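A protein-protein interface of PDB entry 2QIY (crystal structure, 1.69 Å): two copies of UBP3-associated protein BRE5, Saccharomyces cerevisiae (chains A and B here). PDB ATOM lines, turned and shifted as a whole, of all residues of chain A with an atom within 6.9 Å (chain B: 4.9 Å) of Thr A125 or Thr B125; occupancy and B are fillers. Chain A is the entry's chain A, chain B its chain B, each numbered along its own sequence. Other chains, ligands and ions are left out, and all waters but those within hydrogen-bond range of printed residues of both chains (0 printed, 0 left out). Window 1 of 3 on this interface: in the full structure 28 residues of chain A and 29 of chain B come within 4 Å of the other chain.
SD of Met A107 is in hydrogen-bond range of OG1 of Thr B125, 3.1 Å away.
NE2 of Gln A95 sits at hydrogen-bond distance from O of Asp B142.
SG of Cys A123 lies within hydrogen-bond range of SD of Met B107 (3.3 Å).
The side-chain amide oxygen (OD1) of Asn B141 sits close to the side-chain amide oxygen (OE1) of Gln A95 (2.9 Å).
The side-chain amide oxygen (OE1) of Gln B124 lies close to the side-chain carboxylate (OD1) of Asp B142, at 2.9 Å.
N of Thr A125 is in hydrogen-bond range of O of Ile A143.
The backbone NH (N) of Ile A127 sits at hydrogen-bond distance from the backbone carbonyl oxygen (O) of Asn A141.
The backbone NH (N) of Arg A145 sits at hydrogen-bond distance from the backbone carbonyl oxygen (O) of Cys A123 (2.9 Å).
O of Ile B143 is in hydrogen-bond range of N of Thr B125, 2.8 Å away.
The backbone carbonyl oxygen (O) of Asn B141 sits at hydrogen-bond distance from the backbone NH (N) of Ile B127 (3.0 Å).
Among the printed residues, pairs that only touch across the chains: Thr A125 with Met B107 (3.3 Å), Gln A95 with Ile B143 (3.4 Å), Thr A125 with Thr B125 (3.4 Å), Met A107 with Cys B123 (3.5 Å), Ile A143 with Met B107 (3.5 Å), Leu A105 with Ile B143 (3.5 Å), Ile A127 with Ile B127 (3.6 Å), Met A107 with Ile B143 (3.6 Å), Ile A143 with Leu B105 (3.6 Å), Leu A105 with Asn B141 (3.7 Å), Leu A105 with Ile B127 (3.7 Å), Asn A141 with Leu B105 (3.8 Å), Cys A123 with Cys B123 (3.9 Å) and Leu A105 with Thr B125 (3.98 Å).
Thr A125 touches just these residues of chain B: Met B107 (3.3 Å) and Thr B125 (3.4 Å).
Thr B125 touches just these residues of chain A: Leu A105, Met A107 and Thr A125.
Of the printed residues of chain B, Ile A143 touches Leu B105 and Met B107.
Printed residues of chain B within 4 Å of Ile A127: Ile B127 (3.6 Å).
Of the printed residues of chain B, Asn A141 touches Leu B105 (3.8 Å).
Of the printed residues of chain B, Gln A95 touches Asn B141 (2.9 Å), Asp B142 (3.2 Å) and Ile B143 (3.4 Å).
Ala A108 touches none of the printed residues of chain B.
Phe A122 touches none of the printed residues of chain B.
The nearest residue of chain B that does not touch Thr A125 is Leu B105 (4.1 Å).
The nearest printed residue of chain A that does not touch Met B107 is Arg A145 (4.2 Å).
Hydrophobic or aromatic side chains of chain A within 4 Å of the printed part of chain B: Leu A105, Met A107, Ile A127 and Ile A143.
Of the 11 printed residues of chain B, 8 touch a printed residue of chain A.
Printed residues of chain B that touch a printed residue of chain A: Leu B105, Met B107, Cys B123, Thr B125, Ile B127, Asn B141, Asp B142 and Ile B143.
Hydrophobic or aromatic side chains of chain B that line the printed part of chain A: Leu B105, Met B107, Ile B127 and Ile B143.
Along chain B the printed residues that touch a printed residue of chain A span positions 105 to 143.
Among the printed residues, 18 pairs touch across the chains.
Leu A105 touches Thr B125, but with the chains exchanged Thr A125 does not touch Leu B105 (4.1 Å).
Leu A105 touches Asn B141, and with the chains exchanged Asn A141 touches Leu B105.
Met A107 touches Thr B125, and with the chains exchanged Thr A125 touches Met B107.
Thr A125 touches its own counterpart, Thr B125.
11 positions are printed for both chains.
Of the 18 pairs that touch across the chains among the printed residues, 13 have their exchanged pair printed and touching as well.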
ATOM      1  N   TYR A  23      14.164   5.496 -29.452  1.00  0.00           N
ATOM      2  CA  TYR A  23      14.299   6.918 -29.129  1.00  0.00           C
ATOM      3  C   TYR A  23      14.701   7.751 -30.320  1.00  0.00           C
ATOM      4  O   TYR A  23      14.288   8.908 -30.449  1.00  0.00           O
ATOM      5  CB  TYR A  23      15.233   7.153 -27.950  1.00  0.00           C
ATOM      6  CG  TYR A  23      14.719   6.580 -26.648  1.00  0.00           C
ATOM      7  CD1 TYR A  23      13.588   7.110 -26.008  1.00  0.00           C
ATOM      8  CD2 TYR A  23      15.380   5.510 -26.039  1.00  0.00           C
ATOM      9  CE1 TYR A  23      13.116   6.561 -24.789  1.00  0.00           C
ATOM     10  CE2 TYR A  23      14.937   4.976 -24.833  1.00  0.00           C
ATOM     11  CZ  TYR A  23      13.809   5.497 -24.216  1.00  0.00           C
ATOM     12  OH  TYR A  23      13.381   4.963 -23.027  1.00  0.00           O
ATOM     13  N   GLN A  95      14.583  -9.483 -19.186  1.00  0.00           N
ATOM     14  CA  GLN A  95      14.299 -10.920 -18.991  1.00  0.00           C
ATOM     15  C   GLN A  95      13.416 -11.420 -20.126  1.00  0.00           C
ATOM     16  O   GLN A  95      12.707 -10.640 -20.761  1.00  0.00           O
ATOM     17  CB  GLN A  95      13.562 -11.174 -17.671  1.00  0.00           C
ATOM     18  CG  GLN A  95      14.284 -10.771 -16.381  1.00  0.00           C
ATOM     19  CD  GLN A  95      13.394 -10.929 -15.137  1.00  0.00           C
ATOM     20  OE1 GLN A  95      12.164 -11.007 -15.246  1.00  0.00           O
ATOM     21  NE2 GLN A  95      14.012 -10.978 -13.961  1.00  0.00           N
ATOM     22  N   LEU A 105      11.060  -8.692 -21.843  1.00  0.00           N
ATOM     23  CA  LEU A 105      10.780  -7.598 -20.900  1.00  0.00           C
ATOM     24  C   LEU A 105      12.023  -6.747 -20.787  1.00  0.00           C
ATOM     25  O   LEU A 105      13.094  -7.270 -20.470  1.00  0.00           O
ATOM     26  CB  LEU A 105      10.503  -8.201 -19.512  1.00  0.00           C
ATOM     27  CG  LEU A 105       9.675  -7.518 -18.400  1.00  0.00           C
ATOM     28  CD1 LEU A 105      10.077  -7.887 -16.952  1.00  0.00           C
ATOM     29  CD2 LEU A 105       9.278  -6.039 -18.586  1.00  0.00           C
ATOM     30  N   ILE A 106      11.893  -5.439 -21.051  1.00  0.00           N
ATOM     31  CA  ILE A 106      13.011  -4.521 -20.962  1.00  0.00           C
ATOM     32  C   ILE A 106      12.687  -3.392 -19.973  1.00  0.00           C
ATOM     33  O   ILE A 106      11.609  -2.814 -20.022  1.00  0.00           O
ATOM     34  CB  ILE A 106      13.362  -3.896 -22.354  1.00  0.00           C
ATOM     35  CG1 ILE A 106      13.633  -4.988 -23.386  1.00  0.00           C
ATOM     36  CG2 ILE A 106      14.552  -2.941 -22.233  1.00  0.00           C
ATOM     37  CD1 ILE A 106      13.831  -4.450 -24.841  1.00  0.00           C
ATOM     38  N   MET A 107      13.615  -3.069 -19.085  1.00  0.00           N
ATOM     39  CA  MET A 107      13.445  -1.836 -18.299  1.00  0.00           C
ATOM     40  C   MET A 107      14.629  -0.925 -18.525  1.00  0.00           C
ATOM     41  O   MET A 107      15.780  -1.380 -18.459  1.00  0.00           O
ATOM     42  CB  MET A 107      13.416  -2.118 -16.808  1.00  0.00           C
ATOM     43  CG  MET A 107      12.260  -2.848 -16.283  1.00  0.00           C
ATOM     44  SD  MET A 107      12.639  -3.039 -14.522  1.00  0.00           S
ATOM     45  CE  MET A 107      12.344  -1.394 -13.957  1.00  0.00           C
ATOM     46  N   ALA A 108      14.358   0.358 -18.768  1.00  0.00           N
ATOM     47  CA  ALA A 108      15.414   1.337 -18.980  1.00  0.00           C
ATOM     48  C   ALA A 108      15.261   2.440 -17.945  1.00  0.00           C
ATOM     49  O   ALA A 108      14.140   2.746 -17.521  1.00  0.00           O
ATOM     50  CB  ALA A 108      15.290   1.909 -20.358  1.00  0.00           C
ATOM     51  N   PHE A 122      13.602   9.136 -15.180  1.00  0.00           N
ATOM     52  CA  PHE A 122      12.506   8.251 -15.596  1.00  0.00           C
ATOM     53  C   PHE A 122      12.924   6.800 -15.554  1.00  0.00           C
ATOM     54  O   PHE A 122      14.107   6.465 -15.588  1.00  0.00           O
ATOM     55  CB  PHE A 122      12.075   8.583 -17.038  1.00  0.00           C
ATOM     56  CG  PHE A 122      13.039   8.066 -18.092  1.00  0.00           C
ATOM     57  CD1 PHE A 122      12.822   6.807 -18.664  1.00  0.00           C
ATOM     58  CD2 PHE A 122      14.168   8.791 -18.463  1.00  0.00           C
ATOM     59  CE1 PHE A 122      13.686   6.292 -19.606  1.00  0.00           C
ATOM     60  CE2 PHE A 122      15.037   8.294 -19.412  1.00  0.00           C
ATOM     61  CZ  PHE A 122      14.804   7.034 -19.993  1.00  0.00           C
ATOM     62  N   CYS A 123      11.910   5.945 -15.474  1.00  0.00           N
ATOM     63  CA  CYS A 123      12.061   4.541 -15.775  1.00  0.00           C
ATOM     64  C   CYS A 123      11.026   4.193 -16.842  1.00  0.00           C
ATOM     65  O   CYS A 123       9.879   4.673 -16.825  1.00  0.00           O
ATOM     66  CB  CYS A 123      11.864   3.735 -14.517  1.00  0.00           C
ATOM     67  SG  CYS A 123      10.403   4.006 -13.576  1.00  0.00           S
ATOM     68  N   GLN A 124      11.440   3.414 -17.824  1.00  0.00           N
ATOM     69  CA  GLN A 124      10.517   3.072 -18.904  1.00  0.00           C
ATOM     70  C   GLN A 124      10.611   1.572 -19.133  1.00  0.00           C
ATOM     71  O   GLN A 124      11.717   1.030 -19.230  1.00  0.00           O
ATOM     72  CB  GLN A 124      10.828   3.845 -20.204  1.00  0.00           C
ATOM     73  CG  GLN A 124       9.775   3.617 -21.333  1.00  0.00           C
ATOM     74  CD  GLN A 124       9.812   4.667 -22.453  1.00  0.00           C
ATOM     75  OE1 GLN A 124       8.967   4.653 -23.370  1.00  0.00           O
ATOM     76  NE2 GLN A 124      10.766   5.576 -22.385  1.00  0.00           N
ATOM     77  N   THR A 125       9.456   0.912 -19.242  1.00  0.00           N
ATOM     78  CA  THR A 125       9.437  -0.534 -19.402  1.00  0.00           C
ATOM     79  C   THR A 125       8.725  -0.894 -20.685  1.00  0.00           C
ATOM     80  O   THR A 125       7.714  -0.282 -21.016  1.00  0.00           O
ATOM     81  CB  THR A 125       8.723  -1.181 -18.201  1.00  0.00           C
ATOM     82  OG1 THR A 125       9.568  -0.999 -17.058  1.00  0.00           O
ATOM     83  CG2 THR A 125       8.529  -2.635 -18.413  1.00  0.00           C
ATOM     84  N   PHE A 126       9.261  -1.882 -21.390  1.00  0.00           N
ATOM     85  CA  PHE A 126       8.681  -2.388 -22.644  1.00  0.00           C
ATOM     86  C   PHE A 126       8.507  -3.891 -22.603  1.00  0.00           C
ATOM     87  O   PHE A 126       9.280  -4.603 -21.936  1.00  0.00           O
ATOM     88  CB  PHE A 126       9.658  -2.148 -23.784  1.00  0.00           C
ATOM     89  CG  PHE A 126      10.062  -0.715 -23.954  1.00  0.00           C
ATOM     90  CD1 PHE A 126      11.153  -0.200 -23.235  1.00  0.00           C
ATOM     91  CD2 PHE A 126       9.383   0.116 -24.863  1.00  0.00           C
ATOM     92  CE1 PHE A 126      11.542   1.128 -23.411  1.00  0.00           C
ATOM     93  CE2 PHE A 126       9.798   1.440 -25.055  1.00  0.00           C
ATOM     94  CZ  PHE A 126      10.871   1.933 -24.318  1.00  0.00           C
ATOM     95  N   ILE A 127       7.517  -4.383 -23.346  1.00  0.00           N
ATOM     96  CA  ILE A 127       7.440  -5.813 -23.661  1.00  0.00           C
ATOM     97  C   ILE A 127       7.442  -5.952 -25.182  1.00  0.00           C
ATOM     98  O   ILE A 127       6.659  -5.281 -25.869  1.00  0.00           O
ATOM     99  CB  ILE A 127       6.189  -6.513 -23.071  1.00  0.00           C
ATOM    100  CG1 ILE A 127       6.243  -6.461 -21.550  1.00  0.00           C
ATOM    101  CG2 ILE A 127       6.138  -7.996 -23.531  1.00  0.00           C
ATOM    102  CD1 ILE A 127       7.294  -7.311 -20.994  1.00  0.00           C
ATOM    103  N   ILE A 139       6.271  -4.012 -30.205  1.00  0.00           N
ATOM    104  CA  ILE A 139       6.019  -3.530 -28.840  1.00  0.00           C
ATOM    105  C   ILE A 139       4.571  -3.824 -28.428  1.00  0.00           C
ATOM    106  O   ILE A 139       3.646  -3.377 -29.082  1.00  0.00           O
ATOM    107  CB  ILE A 139       6.240  -1.990 -28.720  1.00  0.00           C
ATOM    108  CG1 ILE A 139       7.635  -1.600 -29.179  1.00  0.00           C
ATOM    109  CG2 ILE A 139       6.055  -1.554 -27.283  1.00  0.00           C
ATOM    110  CD1 ILE A 139       7.785  -0.089 -29.403  1.00  0.00           C
ATOM    111  N   ASN A 141       3.723  -3.435 -24.998  1.00  0.00           N
ATOM    112  CA  ASN A 141       3.591  -2.621 -23.782  1.00  0.00           C
ATOM    113  C   ASN A 141       4.723  -1.638 -23.683  1.00  0.00           C
ATOM    114  O   ASN A 141       5.884  -1.969 -23.983  1.00  0.00           O
ATOM    115  CB  ASN A 141       3.636  -3.496 -22.514  1.00  0.00           C
ATOM    116  CG  ASN A 141       2.473  -4.397 -22.408  1.00  0.00           C
ATOM    117  OD1 ASN A 141       1.451  -4.066 -21.781  1.00  0.00           O
ATOM    118  ND2 ASN A 141       2.577  -5.538 -23.046  1.00  0.00           N
ATOM    119  N   ASP A 142       4.384  -0.433 -23.243  1.00  0.00           N
ATOM    120  CA  ASP A 142       5.340   0.662 -23.146  1.00  0.00           C
ATOM    121  C   ASP A 142       4.837   1.586 -22.049  1.00  0.00           C
ATOM    122  O   ASP A 142       3.811   2.228 -22.232  1.00  0.00           O
ATOM    123  CB  ASP A 142       5.358   1.380 -24.497  1.00  0.00           C
ATOM    124  CG  ASP A 142       6.301   2.568 -24.532  1.00  0.00           C
ATOM    125  OD1 ASP A 142       6.831   2.970 -23.478  1.00  0.00           O
ATOM    126  OD2 ASP A 142       6.507   3.091 -25.658  1.00  0.00           O
ATOM    127  N   ILE A 143       5.540   1.612 -20.907  1.00  0.00           N
ATOM    128  CA  ILE A 143       5.126   2.444 -19.753  1.00  0.00           C
ATOM    129  C   ILE A 143       6.299   3.303 -19.327  1.00  0.00           C
ATOM    130  O   ILE A 143       7.405   2.783 -19.101  1.00  0.00           O
ATOM    131  CB  ILE A 143       4.760   1.616 -18.493  1.00  0.00           C
ATOM    132  CG1 ILE A 143       3.644   0.592 -18.770  1.00  0.00           C
ATOM    133  CG2 ILE A 143       4.434   2.593 -17.291  1.00  0.00           C
ATOM    134  CD1 ILE A 143       3.430  -0.369 -17.572  1.00  0.00           C
ATOM    135  N   ILE A 144       6.098   4.624 -19.241  1.00  0.00           N
ATOM    136  CA  ILE A 144       7.102   5.482 -18.608  1.00  0.00           C
ATOM    137  C   ILE A 144       6.576   6.031 -17.270  1.00  0.00           C
ATOM    138  O   ILE A 144       5.388   6.340 -17.128  1.00  0.00           O
ATOM    139  CB  ILE A 144       7.555   6.627 -19.557  1.00  0.00           C
ATOM    140  CG1 ILE A 144       8.804   7.348 -19.013  1.00  0.00           C
ATOM    141  CG2 ILE A 144       6.388   7.614 -19.863  1.00  0.00           C
ATOM    142  CD1 ILE A 144       9.493   8.227 -20.098  1.00  0.00           C
ATOM    143  N   ARG A 145       7.481   6.134 -16.300  1.00  0.00           N
ATOM    144  CA  ARG A 145       7.146   6.728 -15.020  1.00  0.00           C
ATOM    145  C   ARG A 145       8.267   7.713 -14.676  1.00  0.00           C
ATOM    146  O   ARG A 145       9.453   7.347 -14.671  1.00  0.00           O
ATOM    147  CB  ARG A 145       7.010   5.645 -13.924  1.00  0.00           C
ATOM    148  CG  ARG A 145       7.109   6.198 -12.478  1.00  0.00           C
ATOM    149  CD  ARG A 145       6.001   7.180 -12.095  1.00  0.00           C
ATOM    150  NE  ARG A 145       4.650   6.600 -12.205  1.00  0.00           N
ATOM    151  CZ  ARG A 145       3.534   7.210 -11.787  1.00  0.00           C
ATOM    152  NH1 ARG A 145       3.592   8.417 -11.191  1.00  0.00           N
ATOM    153  NH2 ARG A 145       2.351   6.605 -11.905  1.00  0.00           N
ATOM    154  N   LEU B 105       1.276  -6.431 -16.286  1.00  0.00           N
ATOM    155  CA  LEU B 105       2.583  -5.788 -16.143  1.00  0.00           C
ATOM    156  C   LEU B 105       2.439  -4.695 -15.079  1.00  0.00           C
ATOM    157  O   LEU B 105       1.526  -3.874 -15.164  1.00  0.00           O
ATOM    158  CB  LEU B 105       3.004  -5.188 -17.497  1.00  0.00           C
ATOM    159  CG  LEU B 105       4.200  -4.227 -17.452  1.00  0.00           C
ATOM    160  CD1 LEU B 105       5.459  -4.988 -17.057  1.00  0.00           C
ATOM    161  CD2 LEU B 105       4.420  -3.583 -18.847  1.00  0.00           C
ATOM    162  N   ILE B 106       3.308  -4.702 -14.057  1.00  0.00           N
ATOM    163  CA  ILE B 106       3.253  -3.715 -12.962  1.00  0.00           C
ATOM    164  C   ILE B 106       4.614  -3.072 -12.796  1.00  0.00           C
ATOM    165  O   ILE B 106       5.639  -3.773 -12.810  1.00  0.00           O
ATOM    166  CB  ILE B 106       2.883  -4.374 -11.597  1.00  0.00           C
ATOM    167  CG1 ILE B 106       1.553  -5.086 -11.701  1.00  0.00           C
ATOM    168  CG2 ILE B 106       2.854  -3.326 -10.438  1.00  0.00           C
ATOM    169  CD1 ILE B 106       1.242  -5.995 -10.486  1.00  0.00           C
ATOM    170  N   MET B 107       4.634  -1.746 -12.648  1.00  0.00           N
ATOM    171  CA  MET B 107       5.868  -1.031 -12.311  1.00  0.00           C
ATOM    172  C   MET B 107       5.634  -0.297 -11.016  1.00  0.00           C
ATOM    173  O   MET B 107       4.631   0.380 -10.855  1.00  0.00           O
ATOM    174  CB  MET B 107       6.268  -0.012 -13.419  1.00  0.00           C
ATOM    175  CG  MET B 107       7.668   0.616 -13.169  1.00  0.00           C
ATOM    176  SD  MET B 107       8.254   1.677 -14.542  1.00  0.00           S
ATOM    177  CE  MET B 107       7.196   1.002 -15.816  1.00  0.00           C
ATOM    178  N   CYS B 123      13.165   1.283  -8.823  1.00  0.00           N
ATOM    179  CA  CYS B 123      12.012   0.912  -9.660  1.00  0.00           C
ATOM    180  C   CYS B 123      11.965  -0.596  -9.764  1.00  0.00           C
ATOM    181  O   CYS B 123      13.002  -1.262  -9.832  1.00  0.00           O
ATOM    182  CB  CYS B 123      12.069   1.559 -11.017  1.00  0.00           C
ATOM    183  SG  CYS B 123      13.520   1.224 -12.009  1.00  0.00           S
ATOM    184  N   GLN B 124      10.765  -1.154  -9.746  1.00  0.00           N
ATOM    185  CA  GLN B 124      10.660  -2.613  -9.758  1.00  0.00           C
ATOM    186  C   GLN B 124       9.524  -2.962 -10.706  1.00  0.00           C
ATOM    187  O   GLN B 124       8.463  -2.330 -10.649  1.00  0.00           O
ATOM    188  CB  GLN B 124      10.380  -3.167  -8.361  1.00  0.00           C
ATOM    189  CG  GLN B 124      10.324  -4.717  -8.313  1.00  0.00           C
ATOM    190  CD  GLN B 124      10.375  -5.308  -6.912  1.00  0.00           C
ATOM    191  OE1 GLN B 124      10.563  -6.530  -6.736  1.00  0.00           O
ATOM    192  NE2 GLN B 124      10.169  -4.472  -5.911  1.00  0.00           N
ATOM    193  N   THR B 125       9.753  -3.944 -11.568  1.00  0.00           N
ATOM    194  CA  THR B 125       8.693  -4.390 -12.486  1.00  0.00           C
ATOM    195  C   THR B 125       8.363  -5.855 -12.279  1.00  0.00           C
ATOM    196  O   THR B 125       9.267  -6.667 -12.024  1.00  0.00           O
ATOM    197  CB  THR B 125       8.997  -4.130 -13.955  1.00  0.00           C
ATOM    198  OG1 THR B 125      10.152  -4.879 -14.350  1.00  0.00           O
ATOM    199  CG2 THR B 125       9.262  -2.666 -14.141  1.00  0.00           C
ATOM    200  N   PHE B 126       7.068  -6.151 -12.367  1.00  0.00           N
ATOM    201  CA  PHE B 126       6.553  -7.519 -12.254  1.00  0.00           C
ATOM    202  C   PHE B 126       5.693  -7.818 -13.462  1.00  0.00           C
ATOM    203  O   PHE B 126       5.030  -6.927 -14.006  1.00  0.00           O
ATOM    204  CB  PHE B 126       5.627  -7.695 -11.040  1.00  0.00           C
ATOM    205  CG  PHE B 126       6.254  -7.341  -9.723  1.00  0.00           C
ATOM    206  CD1 PHE B 126       6.253  -6.017  -9.272  1.00  0.00           C
ATOM    207  CD2 PHE B 126       6.820  -8.329  -8.934  1.00  0.00           C
ATOM    208  CE1 PHE B 126       6.826  -5.677  -8.047  1.00  0.00           C
ATOM    209  CE2 PHE B 126       7.384  -7.994  -7.684  1.00  0.00           C
ATOM    210  CZ  PHE B 126       7.360  -6.668  -7.254  1.00  0.00           C
ATOM    211  N   ILE B 127       5.627  -9.101 -13.815  1.00  0.00           N
ATOM    212  CA  ILE B 127       4.584  -9.573 -14.707  1.00  0.00           C
ATOM    213  C   ILE B 127       3.898 -10.730 -13.979  1.00  0.00           C
ATOM    214  O   ILE B 127       4.563 -11.644 -13.452  1.00  0.00           O
ATOM    215  CB  ILE B 127       5.136 -10.078 -16.056  1.00  0.00           C
ATOM    216  CG1 ILE B 127       5.815  -8.923 -16.821  1.00  0.00           C
ATOM    217  CG2 ILE B 127       4.004 -10.794 -16.875  1.00  0.00           C
ATOM    218  CD1 ILE B 127       6.424  -9.312 -18.155  1.00  0.00           C
ATOM    219  N   ASN B 141       7.967 -12.732 -13.877  1.00  0.00           N
ATOM    220  CA  ASN B 141       9.090 -11.812 -13.996  1.00  0.00           C
ATOM    221  C   ASN B 141       9.090 -10.828 -12.864  1.00  0.00           C
ATOM    222  O   ASN B 141       8.035 -10.310 -12.465  1.00  0.00           O
ATOM    223  CB  ASN B 141       8.999 -11.015 -15.312  1.00  0.00           C
ATOM    224  CG  ASN B 141       9.087 -11.900 -16.531  1.00  0.00           C
ATOM    225  OD1 ASN B 141      10.166 -12.125 -17.095  1.00  0.00           O
ATOM    226  ND2 ASN B 141       7.957 -12.443 -16.930  1.00  0.00           N
ATOM    227  N   ASP B 142      10.284 -10.554 -12.351  1.00  0.00           N
ATOM    228  CA  ASP B 142      10.437  -9.620 -11.257  1.00  0.00           C
ATOM    229  C   ASP B 142      11.833  -9.031 -11.404  1.00  0.00           C
ATOM    230  O   ASP B 142      12.821  -9.758 -11.286  1.00  0.00           O
ATOM    231  CB  ASP B 142      10.264 -10.422  -9.943  1.00  0.00           C
ATOM    232  CG  ASP B 142      10.615  -9.627  -8.681  1.00  0.00           C
ATOM    233  OD1 ASP B 142      11.104  -8.472  -8.763  1.00  0.00           O
ATOM    234  OD2 ASP B 142      10.381 -10.202  -7.585  1.00  0.00           O
ATOM    235  N   ILE B 143      11.891  -7.733 -11.724  1.00  0.00           N
ATOM    236  CA  ILE B 143      13.188  -7.018 -11.899  1.00  0.00           C
ATOM    237  C   ILE B 143      13.215  -5.799 -11.004  1.00  0.00           C
ATOM    238  O   ILE B 143      12.264  -4.983 -11.043  1.00  0.00           O
ATOM    239  CB  ILE B 143      13.428  -6.527 -13.365  1.00  0.00           C
ATOM    240  CG1 ILE B 143      13.330  -7.659 -14.402  1.00  0.00           C
ATOM    241  CG2 ILE B 143      14.742  -5.740 -13.440  1.00  0.00           C
ATOM    242  CD1 ILE B 143      13.375  -7.182 -15.845  1.00  0.00           C
